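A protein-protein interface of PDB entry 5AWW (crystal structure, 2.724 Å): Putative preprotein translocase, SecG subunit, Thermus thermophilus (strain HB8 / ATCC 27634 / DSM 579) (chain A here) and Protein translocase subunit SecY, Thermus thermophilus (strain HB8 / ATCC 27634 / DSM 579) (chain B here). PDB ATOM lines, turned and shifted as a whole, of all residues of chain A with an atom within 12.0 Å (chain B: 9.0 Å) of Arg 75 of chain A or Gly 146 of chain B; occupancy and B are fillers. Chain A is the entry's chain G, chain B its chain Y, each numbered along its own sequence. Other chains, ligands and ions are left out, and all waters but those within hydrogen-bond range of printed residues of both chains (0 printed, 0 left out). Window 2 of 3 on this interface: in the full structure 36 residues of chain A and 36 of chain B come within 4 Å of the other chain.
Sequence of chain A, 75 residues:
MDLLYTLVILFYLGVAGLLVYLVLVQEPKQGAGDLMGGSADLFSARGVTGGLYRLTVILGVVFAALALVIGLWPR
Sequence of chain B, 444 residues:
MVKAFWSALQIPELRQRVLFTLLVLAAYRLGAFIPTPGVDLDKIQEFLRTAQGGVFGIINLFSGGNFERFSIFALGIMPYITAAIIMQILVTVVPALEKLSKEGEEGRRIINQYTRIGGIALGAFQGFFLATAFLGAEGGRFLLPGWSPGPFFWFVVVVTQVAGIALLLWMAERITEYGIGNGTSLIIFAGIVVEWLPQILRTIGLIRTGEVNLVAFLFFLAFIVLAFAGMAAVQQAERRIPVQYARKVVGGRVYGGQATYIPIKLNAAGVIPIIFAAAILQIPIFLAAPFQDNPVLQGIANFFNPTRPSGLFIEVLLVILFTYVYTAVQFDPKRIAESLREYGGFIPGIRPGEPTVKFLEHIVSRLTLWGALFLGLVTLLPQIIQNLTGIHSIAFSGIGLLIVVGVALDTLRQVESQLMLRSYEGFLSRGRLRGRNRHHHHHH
Hydrophobic or aromatic side chains of chain B that line the printed part of chain A: Pro 145, Trp 147 and Phe 152. Printed residues of chain A that touch a printed residue of chain B: Tyr 5, Ile 9 and Arg 75.
The backbone carbonyl oxygen (O) of Pro 145 of chain B lies within hydrogen-bond range of the guanidinium group (NE) of Arg 75 of chain A (3.1 Å).
OH of Tyr 5 of chain A touches CH2 of Trp 147 of chain B (3.98 Å). Phe 152 of chain B touches Tyr 5 of chain A. Ile 9 of chain A touches Phe 152 of chain B (CD1 to CE1, 3.5 Å). Arg 75 of chain A touches Gly 146 of chain B (CZ to N, 3.9 Å).
Arg 75 of chain A touches two residues of chain B. Gly 146 of chain B touches one residue of chain A. No residue of chain A comes within 4 Å of Leu 144 of chain B. Of chain A, only Tyr 5 (3.98 Å) comes within 4 Å of Trp 147 of chain B. No residue of chain A comes within 4 Å of Ser 148 of chain B. Printed residues of chain B within 4 Å of Tyr 5 of chain A: Trp 147 (3.98 Å) and Phe 152 (3.7 Å). Of the printed residues of chain A, Phe 152 of chain B touches Tyr 5 (3.7 Å) and Ile 9 (3.5 Å). Of the printed residues of chain B, Ile 9 of chain A touches Phe 152 (3.5 Å). Ile 70 of chain A touches none of the printed residues of chain B. The nearest residue of chain A that does not touch Gly 146 of chain B is Pro 74 of chain A (7.3 Å). The nearest printed residue of chain B that does not touch Tyr 5 of chain A is Gly 38 of chain B (7.7 Å).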
ATOM      1  N   MET A   1       7.395   4.464 -25.697  1.00  0.00           N
ATOM      2  CA  MET A   1       7.502   5.528 -24.705  1.00  0.00           C
ATOM      3  C   MET A   1       6.632   5.251 -23.477  1.00  0.00           C
ATOM      4  O   MET A   1       5.539   5.801 -23.336  1.00  0.00           O
ATOM      5  CB  MET A   1       7.124   6.876 -25.328  1.00  0.00           C
ATOM      6  CG  MET A   1       8.102   7.358 -26.391  1.00  0.00           C
ATOM      7  SD  MET A   1       7.719   8.997 -27.040  1.00  0.00           S
ATOM      8  CE  MET A   1       9.193   9.333 -27.994  1.00  0.00           C
ATOM      9  N   ASP A   2       7.130   4.389 -22.594  1.00  0.00           N
ATOM     10  CA  ASP A   2       6.453   4.083 -21.336  1.00  0.00           C
ATOM     11  C   ASP A   2       7.017   4.929 -20.206  1.00  0.00           C
ATOM     12  O   ASP A   2       6.294   5.694 -19.571  1.00  0.00           O
ATOM     13  CB  ASP A   2       6.596   2.599 -20.988  1.00  0.00           C
ATOM     14  CG  ASP A   2       5.998   2.255 -19.634  1.00  0.00           C
ATOM     15  OD1 ASP A   2       4.956   2.843 -19.277  1.00  0.00           O
ATOM     16  OD2 ASP A   2       6.572   1.395 -18.930  1.00  0.00           O
ATOM     17  N   LEU A   3       8.315   4.775 -19.963  1.00  0.00           N
ATOM     18  CA  LEU A   3       9.003   5.493 -18.899  1.00  0.00           C
ATOM     19  C   LEU A   3       8.907   6.999 -19.085  1.00  0.00           C
ATOM     20  O   LEU A   3       8.608   7.728 -18.144  1.00  0.00           O
ATOM     21  CB  LEU A   3      10.472   5.067 -18.835  1.00  0.00           C
ATOM     22  CG  LEU A   3      11.383   5.841 -17.879  1.00  0.00           C
ATOM     23  CD1 LEU A   3      10.962   5.641 -16.429  1.00  0.00           C
ATOM     24  CD2 LEU A   3      12.829   5.428 -18.083  1.00  0.00           C
ATOM     25  N   LEU A   4       9.157   7.457 -20.308  1.00  0.00           N
ATOM     26  CA  LEU A   4       9.137   8.883 -20.613  1.00  0.00           C
ATOM     27  C   LEU A   4       7.760   9.481 -20.350  1.00  0.00           C
ATOM     28  O   LEU A   4       7.623  10.468 -19.620  1.00  0.00           O
ATOM     29  CB  LEU A   4       9.550   9.119 -22.066  1.00  0.00           C
ATOM     30  CG  LEU A   4       9.671  10.580 -22.495  1.00  0.00           C
ATOM     31  CD1 LEU A   4      10.654  11.310 -21.599  1.00  0.00           C
ATOM     32  CD2 LEU A   4      10.094  10.678 -23.950  1.00  0.00           C
ATOM     33  N   TYR A   5       6.744   8.863 -20.944  1.00  0.00           N
ATOM     34  CA  TYR A   5       5.362   9.298 -20.784  1.00  0.00           C
ATOM     35  C   TYR A   5       4.940   9.252 -19.320  1.00  0.00           C
ATOM     36  O   TYR A   5       4.246  10.148 -18.840  1.00  0.00           O
ATOM     37  CB  TYR A   5       4.434   8.428 -21.633  1.00  0.00           C
ATOM     38  CG  TYR A   5       3.026   8.958 -21.754  1.00  0.00           C
ATOM     39  CD1 TYR A   5       2.789  10.277 -22.114  1.00  0.00           C
ATOM     40  CD2 TYR A   5       1.930   8.131 -21.535  1.00  0.00           C
ATOM     41  CE1 TYR A   5       1.501  10.764 -22.235  1.00  0.00           C
ATOM     42  CE2 TYR A   5       0.638   8.610 -21.657  1.00  0.00           C
ATOM     43  CZ  TYR A   5       0.430   9.927 -22.006  1.00  0.00           C
ATOM     44  OH  TYR A   5      -0.853  10.410 -22.130  1.00  0.00           O
ATOM     45  N   THR A   6       5.367   8.207 -18.618  1.00  0.00           N
ATOM     46  CA  THR A   6       5.071   8.069 -17.198  1.00  0.00           C
ATOM     47  C   THR A   6       5.690   9.213 -16.407  1.00  0.00           C
ATOM     48  O   THR A   6       5.087   9.715 -15.464  1.00  0.00           O
ATOM     49  CB  THR A   6       5.580   6.731 -16.637  1.00  0.00           C
ATOM     50  OG1 THR A   6       4.983   5.648 -17.361  1.00  0.00           O
ATOM     51  CG2 THR A   6       5.231   6.600 -15.162  1.00  0.00           C
ATOM     52  N   ILE A   9       3.684  12.346 -17.026  1.00  0.00           N
ATOM     53  CA  ILE A   9       2.449  12.267 -16.258  1.00  0.00           C
ATOM     54  C   ILE A   9       2.714  12.532 -14.782  1.00  0.00           C
ATOM     55  O   ILE A   9       1.944  13.232 -14.125  1.00  0.00           O
ATOM     56  CB  ILE A   9       1.768  10.899 -16.433  1.00  0.00           C
ATOM     57  CG1 ILE A   9       1.286  10.738 -17.874  1.00  0.00           C
ATOM     58  CG2 ILE A   9       0.594  10.755 -15.479  1.00  0.00           C
ATOM     59  CD1 ILE A   9       1.081   9.305 -18.279  1.00  0.00           C
ATOM     60  N   LEU A  68      -1.172  20.775 -22.640  1.00  0.00           N
ATOM     61  CA  LEU A  68      -0.979  20.831 -24.084  1.00  0.00           C
ATOM     62  C   LEU A  68       0.002  19.750 -24.553  1.00  0.00           C
ATOM     63  O   LEU A  68      -0.169  19.170 -25.627  1.00  0.00           O
ATOM     64  CB  LEU A  68      -0.491  22.221 -24.509  1.00  0.00           C
ATOM     65  CG  LEU A  68      -1.481  23.378 -24.314  1.00  0.00           C
ATOM     66  CD1 LEU A  68      -1.001  24.654 -25.002  1.00  0.00           C
ATOM     67  CD2 LEU A  68      -2.868  22.992 -24.801  1.00  0.00           C
ATOM     68  N   VAL A  69       1.020  19.473 -23.742  1.00  0.00           N
ATOM     69  CA  VAL A  69       2.010  18.452 -24.072  1.00  0.00           C
ATOM     70  C   VAL A  69       1.378  17.062 -24.089  1.00  0.00           C
ATOM     71  O   VAL A  69       1.543  16.312 -25.053  1.00  0.00           O
ATOM     72  CB  VAL A  69       3.203  18.467 -23.081  1.00  0.00           C
ATOM     73  CG1 VAL A  69       3.944  17.134 -23.098  1.00  0.00           C
ATOM     74  CG2 VAL A  69       4.153  19.609 -23.406  1.00  0.00           C
ATOM     75  N   ILE A  70       0.651  16.727 -23.027  1.00  0.00           N
ATOM     76  CA  ILE A  70      -0.028  15.437 -22.951  1.00  0.00           C
ATOM     77  C   ILE A  70      -1.062  15.315 -24.066  1.00  0.00           C
ATOM     78  O   ILE A  70      -1.254  14.238 -24.633  1.00  0.00           O
ATOM     79  CB  ILE A  70      -0.705  15.236 -21.585  1.00  0.00           C
ATOM     80  CG1 ILE A  70       0.336  15.315 -20.469  1.00  0.00           C
ATOM     81  CG2 ILE A  70      -1.425  13.898 -21.530  1.00  0.00           C
ATOM     82  CD1 ILE A  70      -0.241  15.181 -19.084  1.00  0.00           C
ATOM     83  N   GLY A  71      -1.713  16.429 -24.385  1.00  0.00           N
ATOM     84  CA  GLY A  71      -2.649  16.466 -25.493  1.00  0.00           C
ATOM     85  C   GLY A  71      -2.000  16.179 -26.837  1.00  0.00           C
ATOM     86  O   GLY A  71      -2.573  15.487 -27.675  1.00  0.00           O
ATOM     87  N   LEU A  72      -0.797  16.705 -27.045  1.00  0.00           N
ATOM     88  CA  LEU A  72      -0.110  16.528 -28.321  1.00  0.00           C
ATOM     89  C   LEU A  72       0.669  15.220 -28.395  1.00  0.00           C
ATOM     90  O   LEU A  72       1.261  14.903 -29.427  1.00  0.00           O
ATOM     91  CB  LEU A  72       0.841  17.701 -28.585  1.00  0.00           C
ATOM     92  CG  LEU A  72       0.202  19.039 -28.959  1.00  0.00           C
ATOM     93  CD1 LEU A  72       1.271  20.096 -29.178  1.00  0.00           C
ATOM     94  CD2 LEU A  72      -0.670  18.892 -30.197  1.00  0.00           C
ATOM     95  N   TRP A  73       0.667  14.461 -27.304  1.00  0.00           N
ATOM     96  CA  TRP A  73       1.457  13.235 -27.228  1.00  0.00           C
ATOM     97  C   TRP A  73       0.972  12.191 -28.232  1.00  0.00           C
ATOM     98  O   TRP A  73      -0.231  11.966 -28.370  1.00  0.00           O
ATOM     99  CB  TRP A  73       1.418  12.664 -25.810  1.00  0.00           C
ATOM    100  CG  TRP A  73       2.596  11.799 -25.480  1.00  0.00           C
ATOM    101  CD1 TRP A  73       2.691  10.448 -25.637  1.00  0.00           C
ATOM    102  CD2 TRP A  73       3.851  12.229 -24.937  1.00  0.00           C
ATOM    103  NE1 TRP A  73       3.927  10.009 -25.226  1.00  0.00           N
ATOM    104  CE2 TRP A  73       4.658  11.082 -24.791  1.00  0.00           C
ATOM    105  CE3 TRP A  73       4.371  13.472 -24.560  1.00  0.00           C
ATOM    106  CZ2 TRP A  73       5.955  11.141 -24.284  1.00  0.00           C
ATOM    107  CZ3 TRP A  73       5.661  13.527 -24.056  1.00  0.00           C
ATOM    108  CH2 TRP A  73       6.438  12.368 -23.923  1.00  0.00           C
ATOM    109  N   PRO A  74       1.916  11.556 -28.946  1.00  0.00           N
ATOM    110  CA  PRO A  74       1.633  10.541 -29.969  1.00  0.00           C
ATOM    111  C   PRO A  74       0.929   9.309 -29.409  1.00  0.00           C
ATOM    112  O   PRO A  74       0.851   9.142 -28.191  1.00  0.00           O
ATOM    113  CB  PRO A  74       3.024  10.172 -30.494  1.00  0.00           C
ATOM    114  CG  PRO A  74       3.883  11.346 -30.161  1.00  0.00           C
ATOM    115  CD  PRO A  74       3.356  11.855 -28.858  1.00  0.00           C
ATOM    116  N   ARG A  75       0.430   8.458 -30.301  1.00  0.00           N
ATOM    117  CA  ARG A  75      -0.302   7.255 -29.913  1.00  0.00           C
ATOM    118  C   ARG A  75       0.526   6.328 -29.028  1.00  0.00           C
ATOM    119  O   ARG A  75      -0.022   5.561 -28.236  1.00  0.00           O
ATOM    120  CB  ARG A  75      -0.765   6.497 -31.157  1.00  0.00           C
ATOM    121  CG  ARG A  75      -1.782   7.237 -32.007  1.00  0.00           C
ATOM    122  CD  ARG A  75      -3.120   7.346 -31.298  1.00  0.00           C
ATOM    123  NE  ARG A  75      -4.229   7.395 -32.247  1.00  0.00           N
ATOM    124  CZ  ARG A  75      -4.858   6.320 -32.713  1.00  0.00           C
ATOM    125  NH1 ARG A  75      -5.855   6.453 -33.575  1.00  0.00           N
ATOM    126  NH2 ARG A  75      -4.487   5.111 -32.315  1.00  0.00           N
ATOM    127  OXT ARG A  75       1.756   6.321 -29.083  1.00  0.00           O
ATOM    128  N   GLY B  38      -7.562  13.667 -24.088  1.00  0.00           N
ATOM    129  CA  GLY B  38      -8.401  12.508 -24.331  1.00  0.00           C
ATOM    130  C   GLY B  38      -9.839  12.816 -24.691  1.00  0.00           C
ATOM    131  O   GLY B  38     -10.595  11.920 -25.070  1.00  0.00           O
ATOM    132  N   LEU B 143     -14.489  10.356 -26.492  1.00  0.00           N
ATOM    133  CA  LEU B 143     -13.049  10.160 -26.390  1.00  0.00           C
ATOM    134  C   LEU B 143     -12.344  10.415 -27.717  1.00  0.00           C
ATOM    135  O   LEU B 143     -12.972  10.446 -28.776  1.00  0.00           O
ATOM    136  CB  LEU B 143     -12.727   8.747 -25.898  1.00  0.00           C
ATOM    137  CG  LEU B 143     -13.190   8.365 -24.491  1.00  0.00           C
ATOM    138  CD1 LEU B 143     -12.623   7.012 -24.094  1.00  0.00           C
ATOM    139  CD2 LEU B 143     -12.796   9.426 -23.481  1.00  0.00           C
ATOM    140  N   LEU B 144     -11.031  10.598 -27.642  1.00  0.00           N
ATOM    141  CA  LEU B 144     -10.199  10.789 -28.824  1.00  0.00           C
ATOM    142  C   LEU B 144      -9.580   9.465 -29.264  1.00  0.00           C
ATOM    143  O   LEU B 144      -9.442   8.545 -28.455  1.00  0.00           O
ATOM    144  CB  LEU B 144      -9.104  11.822 -28.540  1.00  0.00           C
ATOM    145  CG  LEU B 144      -9.552  13.282 -28.561  1.00  0.00           C
ATOM    146  CD1 LEU B 144      -8.417  14.203 -28.150  1.00  0.00           C
ATOM    147  CD2 LEU B 144     -10.066  13.647 -29.943  1.00  0.00           C
ATOM    148  N   PRO B 145      -9.222   9.356 -30.554  1.00  0.00           N
ATOM    149  CA  PRO B 145      -8.530   8.171 -31.075  1.00  0.00           C
ATOM    150  C   PRO B 145      -7.243   7.859 -30.310  1.00  0.00           C
ATOM    151  O   PRO B 145      -6.311   8.664 -30.319  1.00  0.00           O
ATOM    152  CB  PRO B 145      -8.222   8.557 -32.522  1.00  0.00           C
ATOM    153  CG  PRO B 145      -9.290   9.522 -32.880  1.00  0.00           C
ATOM    154  CD  PRO B 145      -9.571  10.302 -31.629  1.00  0.00           C
ATOM    155  N   GLY B 146      -7.202   6.704 -29.655  1.00  0.00           N
ATOM    156  CA  GLY B 146      -6.051   6.312 -28.863  1.00  0.00           C
ATOM    157  C   GLY B 146      -6.356   6.323 -27.377  1.00  0.00           C
ATOM    158  O   GLY B 146      -5.492   6.029 -26.549  1.00  0.00           O
ATOM    159  N   TRP B 147      -7.596   6.669 -27.041  1.00  0.00           N
ATOM    160  CA  TRP B 147      -8.032   6.728 -25.651  1.00  0.00           C
ATOM    161  C   TRP B 147      -9.165   5.746 -25.385  1.00  0.00           C
ATOM    162  O   TRP B 147     -10.077   5.604 -26.197  1.00  0.00           O
ATOM    163  CB  TRP B 147      -8.477   8.145 -25.288  1.00  0.00           C
ATOM    164  CG  TRP B 147      -7.374   9.156 -25.306  1.00  0.00           C
ATOM    165  CD1 TRP B 147      -6.911   9.845 -26.388  1.00  0.00           C
ATOM    166  CD2 TRP B 147      -6.600   9.601 -24.186  1.00  0.00           C
ATOM    167  NE1 TRP B 147      -5.895  10.689 -26.011  1.00  0.00           N
ATOM    168  CE2 TRP B 147      -5.684  10.557 -24.665  1.00  0.00           C
ATOM    169  CE3 TRP B 147      -6.595   9.282 -22.824  1.00  0.00           C
ATOM    170  CZ2 TRP B 147      -4.771  11.199 -23.831  1.00  0.00           C
ATOM    171  CZ3 TRP B 147      -5.687   9.920 -21.999  1.00  0.00           C
ATOM    172  CH2 TRP B 147      -4.788  10.867 -22.505  1.00  0.00           C
ATOM    173  N   SER B 148      -9.105   5.078 -24.238  1.00  0.00           N
ATOM    174  CA  SER B 148     -10.117   4.101 -23.860  1.00  0.00           C
ATOM    175  C   SER B 148     -10.655   4.397 -22.461  1.00  0.00           C
ATOM    176  O   SER B 148      -9.916   4.872 -21.600  1.00  0.00           O
ATOM    177  CB  SER B 148      -9.540   2.685 -23.920  1.00  0.00           C
ATOM    178  OG  SER B 148      -8.499   2.520 -22.975  1.00  0.00           O
ATOM    179  N   PRO B 149     -11.949   4.118 -22.232  1.00  0.00           N
ATOM    180  CA  PRO B 149     -12.579   4.399 -20.937  1.00  0.00           C
ATOM    181  C   PRO B 149     -12.014   3.543 -19.811  1.00  0.00           C
ATOM    182  O   PRO B 149     -12.495   2.438 -19.568  1.00  0.00           O
ATOM    183  CB  PRO B 149     -14.054   4.067 -21.186  1.00  0.00           C
ATOM    184  CG  PRO B 149     -14.034   3.087 -22.308  1.00  0.00           C
ATOM    185  CD  PRO B 149     -12.893   3.506 -23.184  1.00  0.00           C
ATOM    186  N   PHE B 152      -6.903   5.183 -16.219  1.00  0.00           N
ATOM    187  CA  PHE B 152      -5.885   6.142 -16.630  1.00  0.00           C
ATOM    188  C   PHE B 152      -6.517   7.453 -17.071  1.00  0.00           C
ATOM    189  O   PHE B 152      -6.110   8.525 -16.624  1.00  0.00           O
ATOM    190  CB  PHE B 152      -5.015   5.586 -17.754  1.00  0.00           C
ATOM    191  CG  PHE B 152      -4.057   6.595 -18.313  1.00  0.00           C
ATOM    192  CD1 PHE B 152      -3.011   7.073 -17.539  1.00  0.00           C
ATOM    193  CD2 PHE B 152      -4.211   7.083 -19.600  1.00  0.00           C
ATOM    194  CE1 PHE B 152      -2.130   8.011 -18.041  1.00  0.00           C
ATOM    195  CE2 PHE B 152      -3.330   8.022 -20.109  1.00  0.00           C
ATOM    196  CZ  PHE B 152      -2.290   8.486 -19.328  1.00  0.00           C
ATOM    197  N   PHE B 153      -7.509   7.356 -17.952  1.00  0.00           N
ATOM    198  CA  PHE B 153      -8.239   8.523 -18.434  1.00  0.00           C
ATOM    199  C   PHE B 153      -8.945   9.251 -17.293  1.00  0.00           C
ATOM    200  O   PHE B 153      -8.925  10.481 -17.224  1.00  0.00           O
ATOM    201  CB  PHE B 153      -9.252   8.109 -19.500  1.00  0.00           C
ATOM    202  CG  PHE B 153     -10.196   9.207 -19.898  1.00  0.00           C
ATOM    203  CD1 PHE B 153      -9.768  10.250 -20.705  1.00  0.00           C
ATOM    204  CD2 PHE B 153     -11.517   9.191 -19.474  1.00  0.00           C
ATOM    205  CE1 PHE B 153     -10.636  11.263 -21.074  1.00  0.00           C
ATOM    206  CE2 PHE B 153     -12.391  10.198 -19.840  1.00  0.00           C
ATOM    207  CZ  PHE B 153     -11.949  11.236 -20.641  1.00  0.00           C
